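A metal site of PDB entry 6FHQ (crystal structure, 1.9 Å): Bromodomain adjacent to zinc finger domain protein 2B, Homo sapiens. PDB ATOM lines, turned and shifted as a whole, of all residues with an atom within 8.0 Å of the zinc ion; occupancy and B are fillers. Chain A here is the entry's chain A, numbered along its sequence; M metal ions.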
ATOM      1  N   LEU A  23      10.415  15.004  23.707  1.00  0.00           N
ATOM      2  CA  LEU A  23      11.450  14.687  22.716  1.00  0.00           C
ATOM      3  C   LEU A  23      11.314  13.294  22.303  1.00  0.00           C
ATOM      4  O   LEU A  23      11.393  12.395  23.164  1.00  0.00           O
ATOM      5  CB  LEU A  23      12.816  14.856  23.346  1.00  0.00           C
ATOM      6  CG  LEU A  23      13.081  16.253  23.904  1.00  0.00           C
ATOM      7  CD1 LEU A  23      14.555  16.278  24.387  1.00  0.00           C
ATOM      8  CD2 LEU A  23      12.836  17.289  22.810  1.00  0.00           C
ATOM      9  N   CYS A  24      11.102  13.072  21.024  1.00  0.00           N
ATOM     10  CA  CYS A  24      10.886  11.715  20.556  1.00  0.00           C
ATOM     11  C   CYS A  24      12.203  10.914  20.583  1.00  0.00           C
ATOM     12  O   CYS A  24      13.214  11.330  19.977  1.00  0.00           O
ATOM     13  CB  CYS A  24      10.280  11.714  19.195  1.00  0.00           C
ATOM     14  SG  CYS A  24      10.053  10.052  18.486  1.00  0.00           S
ATOM     15  N   ASP A  25      12.185   9.800  21.299  1.00  0.00           N
ATOM     16  CA  ASP A  25      13.364   8.916  21.352  1.00  0.00           C
ATOM     17  C   ASP A  25      13.553   8.215  20.031  1.00  0.00           C
ATOM     18  O   ASP A  25      14.616   7.638  19.769  1.00  0.00           O
ATOM     19  CB  ASP A  25      13.195   7.871  22.451  1.00  0.00           C
ATOM     20  CG  ASP A  25      13.344   8.475  23.825  1.00  0.00           C
ATOM     21  OD1 ASP A  25      14.478   8.783  24.211  1.00  0.00           O
ATOM     22  OD2 ASP A  25      12.308   8.749  24.474  1.00  0.00           O
ATOM     23  N   GLY A  26      12.521   8.251  19.171  1.00  0.00           N
ATOM     24  CA  GLY A  26      12.604   7.714  17.826  1.00  0.00           C
ATOM     25  C   GLY A  26      13.384   8.570  16.872  1.00  0.00           C
ATOM     26  O   GLY A  26      14.336   8.091  16.264  1.00  0.00           O
ATOM     27  N   CYS A  27      12.910   9.784  16.639  1.00  0.00           N
ATOM     28  CA  CYS A  27      13.389  10.618  15.534  1.00  0.00           C
ATOM     29  C   CYS A  27      14.023  11.896  16.066  1.00  0.00           C
ATOM     30  O   CYS A  27      14.298  12.772  15.315  1.00  0.00           O
ATOM     31  CB  CYS A  27      12.215  10.992  14.618  1.00  0.00           C
ATOM     32  SG  CYS A  27      10.978  12.008  15.472  1.00  0.00           S
ATOM     33  N   ASP A  28      14.122  12.023  17.389  1.00  0.00           N
ATOM     34  CA  ASP A  28      14.608  13.236  18.066  1.00  0.00           C
ATOM     35  C   ASP A  28      13.921  14.602  17.817  1.00  0.00           C
ATOM     36  O   ASP A  28      14.417  15.624  18.307  1.00  0.00           O
ATOM     37  CB  ASP A  28      16.136  13.354  17.874  1.00  0.00           C
ATOM     38  CG  ASP A  28      16.849  12.132  18.358  1.00  0.00           C
ATOM     39  OD1 ASP A  28      16.816  11.878  19.580  1.00  0.00           O
ATOM     40  OD2 ASP A  28      17.260  11.329  17.502  1.00  0.00           O
ATOM     41  N   LYS A  29      12.753  14.633  17.193  1.00  0.00           N
ATOM     42  CA  LYS A  29      12.006  15.888  17.049  1.00  0.00           C
ATOM     43  C   LYS A  29      11.278  16.218  18.370  1.00  0.00           C
ATOM     44  O   LYS A  29      11.092  15.344  19.187  1.00  0.00           O
ATOM     45  CB  LYS A  29      11.043  15.761  15.924  1.00  0.00           C
ATOM     46  CG  LYS A  29      11.773  15.614  14.587  1.00  0.00           C
ATOM     47  CD  LYS A  29      10.816  15.802  13.437  1.00  0.00           C
ATOM     48  CE  LYS A  29      11.573  16.183  12.140  1.00  0.00           C
ATOM     49  NZ  LYS A  29      10.712  15.852  10.955  1.00  0.00           N
ATOM     50  N   GLY A  30      10.879  17.487  18.548  1.00  0.00           N
ATOM     51  CA  GLY A  30      10.167  17.932  19.742  1.00  0.00           C
ATOM     52  C   GLY A  30       8.783  18.466  19.487  1.00  0.00           C
ATOM     53  O   GLY A  30       8.456  18.926  18.407  1.00  0.00           O
ATOM     54  N   TRP A  48       9.354   8.699  25.179  1.00  0.00           N
ATOM     55  CA  TRP A  48       8.301   9.248  24.321  1.00  0.00           C
ATOM     56  C   TRP A  48       8.624   8.892  22.873  1.00  0.00           C
ATOM     57  O   TRP A  48       9.744   9.077  22.449  1.00  0.00           O
ATOM     58  CB  TRP A  48       8.322  10.757  24.411  1.00  0.00           C
ATOM     59  CG  TRP A  48       7.343  11.408  23.532  1.00  0.00           C
ATOM     60  CD1 TRP A  48       7.608  12.237  22.481  1.00  0.00           C
ATOM     61  CD2 TRP A  48       5.969  11.208  23.554  1.00  0.00           C
ATOM     62  NE1 TRP A  48       6.469  12.596  21.889  1.00  0.00           N
ATOM     63  CE2 TRP A  48       5.426  11.948  22.495  1.00  0.00           C
ATOM     64  CE3 TRP A  48       5.125  10.421  24.331  1.00  0.00           C
ATOM     65  CZ2 TRP A  48       4.080  12.028  22.257  1.00  0.00           C
ATOM     66  CZ3 TRP A  48       3.776  10.472  24.075  1.00  0.00           C
ATOM     67  CH2 TRP A  48       3.252  11.279  23.049  1.00  0.00           C
ATOM     68  N   PHE A  49       7.652   8.327  22.168  1.00  0.00           N
ATOM     69  CA  PHE A  49       7.687   8.202  20.732  1.00  0.00           C
ATOM     70  C   PHE A  49       6.541   9.005  20.132  1.00  0.00           C
ATOM     71  O   PHE A  49       5.362   8.881  20.557  1.00  0.00           O
ATOM     72  CB  PHE A  49       7.600   6.746  20.348  1.00  0.00           C
ATOM     73  CG  PHE A  49       8.805   5.963  20.769  1.00  0.00           C
ATOM     74  CD1 PHE A  49       9.986   6.021  20.026  1.00  0.00           C
ATOM     75  CD2 PHE A  49       8.783   5.228  21.973  1.00  0.00           C
ATOM     76  CE1 PHE A  49      11.123   5.365  20.486  1.00  0.00           C
ATOM     77  CE2 PHE A  49       9.936   4.546  22.391  1.00  0.00           C
ATOM     78  CZ  PHE A  49      11.077   4.632  21.672  1.00  0.00           C
ATOM     79  N   CYS A  50       6.844   9.762  19.089  1.00  0.00           N
ATOM     80  CA  CYS A  50       5.870  10.707  18.557  1.00  0.00           C
ATOM     81  C   CYS A  50       4.901   9.992  17.663  1.00  0.00           C
ATOM     82  O   CYS A  50       5.183   8.900  17.155  1.00  0.00           O
ATOM     83  CB  CYS A  50       6.599  11.844  17.808  1.00  0.00           C
ATOM     84  SG  CYS A  50       7.204  11.371  16.231  1.00  0.00           S
ATOM     85  N   PRO A  51       3.765  10.632  17.353  1.00  0.00           N
ATOM     86  CA  PRO A  51       2.779   9.984  16.591  1.00  0.00           C
ATOM     87  C   PRO A  51       3.300   9.474  15.261  1.00  0.00           C
ATOM     88  O   PRO A  51       2.865   8.430  14.789  1.00  0.00           O
ATOM     89  CB  PRO A  51       1.766  11.120  16.338  1.00  0.00           C
ATOM     90  CG  PRO A  51       1.855  11.912  17.562  1.00  0.00           C
ATOM     91  CD  PRO A  51       3.318  11.989  17.742  1.00  0.00           C
ATOM     92  N   ALA A  52       4.154  10.264  14.641  1.00  0.00           N
ATOM     93  CA  ALA A  52       4.653   9.933  13.327  1.00  0.00           C
ATOM     94  C   ALA A  52       5.446   8.597  13.383  1.00  0.00           C
ATOM     95  O   ALA A  52       5.200   7.726  12.620  1.00  0.00           O
ATOM     96  CB  ALA A  52       5.544  11.095  12.800  1.00  0.00           C
ATOM     97  N   CYS A  53       6.289   8.444  14.403  1.00  0.00           N
ATOM     98  CA  CYS A  53       7.088   7.223  14.601  1.00  0.00           C
ATOM     99  C   CYS A  53       6.239   5.983  14.926  1.00  0.00           C
ATOM    100  O   CYS A  53       6.473   4.944  14.388  1.00  0.00           O
ATOM    101  CB  CYS A  53       8.130   7.449  15.646  1.00  0.00           C
ATOM    102  SG  CYS A  53       9.512   8.507  15.047  1.00  0.00           S
ATOM    103  N   ILE A  54       5.235   6.134  15.772  1.00  0.00           N
ATOM    104  CA  ILE A  54       4.282   5.046  16.086  1.00  0.00           C
ATOM    105  C   ILE A  54       3.507   4.525  14.882  1.00  0.00           C
ATOM    106  O   ILE A  54       3.463   3.317  14.619  1.00  0.00           O
ATOM    107  CB  ILE A  54       3.263   5.526  17.144  1.00  0.00           C
ATOM    108  CG1 ILE A  54       3.969   5.886  18.442  1.00  0.00           C
ATOM    109  CG2 ILE A  54       2.214   4.440  17.437  1.00  0.00           C
ATOM    110  CD1 ILE A  54       4.779   4.750  19.057  1.00  0.00           C
ATOM    111  N   LYS A  56       4.513   4.846  11.640  1.00  0.00           N
ATOM    112  CA  LYS A  56       5.495   4.128  10.829  1.00  0.00           C
ATOM    113  C   LYS A  56       5.817   2.747  11.405  1.00  0.00           C
ATOM    114  O   LYS A  56       5.955   1.820  10.671  1.00  0.00           O
ATOM    115  CB  LYS A  56       6.821   4.890  10.731  1.00  0.00           C
ATOM    116  CG  LYS A  56       6.817   6.106   9.821  1.00  0.00           C
ATOM    117  CD  LYS A  56       8.150   6.843   9.864  1.00  0.00           C
ATOM    118  CE  LYS A  56       9.294   5.940   9.352  1.00  0.00           C
ATOM    119  NZ  LYS A  56      10.612   6.623   9.240  1.00  0.00           N
HETATM  120 ZN    ZN M   1       9.403  10.526  16.270  1.00  0.00          ZN
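The backbone NH of Cys 24 is in hydrogen-bond range of the backbone carbonyl oxygen of Lys 29 (2.9 Å).
SG of Cys 24 lies close to N of Gly 26 (3.1 Å).
SG of Cys 27 lies close to N of Lys 29 (3.6 Å).
SG of Cys 50 sits close to N of Ala 52.
Of the 16 residues printed, 4 come within 4 Å of the zinc ion.
The nearest printed residue that does not touch the zinc ion is Gly 26 (4.5 Å).
The zinc ion is bound by SG of Cys 27 (2.3 Å), SG of Cys 50 (2.4 Å), SG of Cys 24 (2.4 Å) and SG of Cys 53 (2.4 Å).
The zinc ion has four donor atoms within binding distance.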
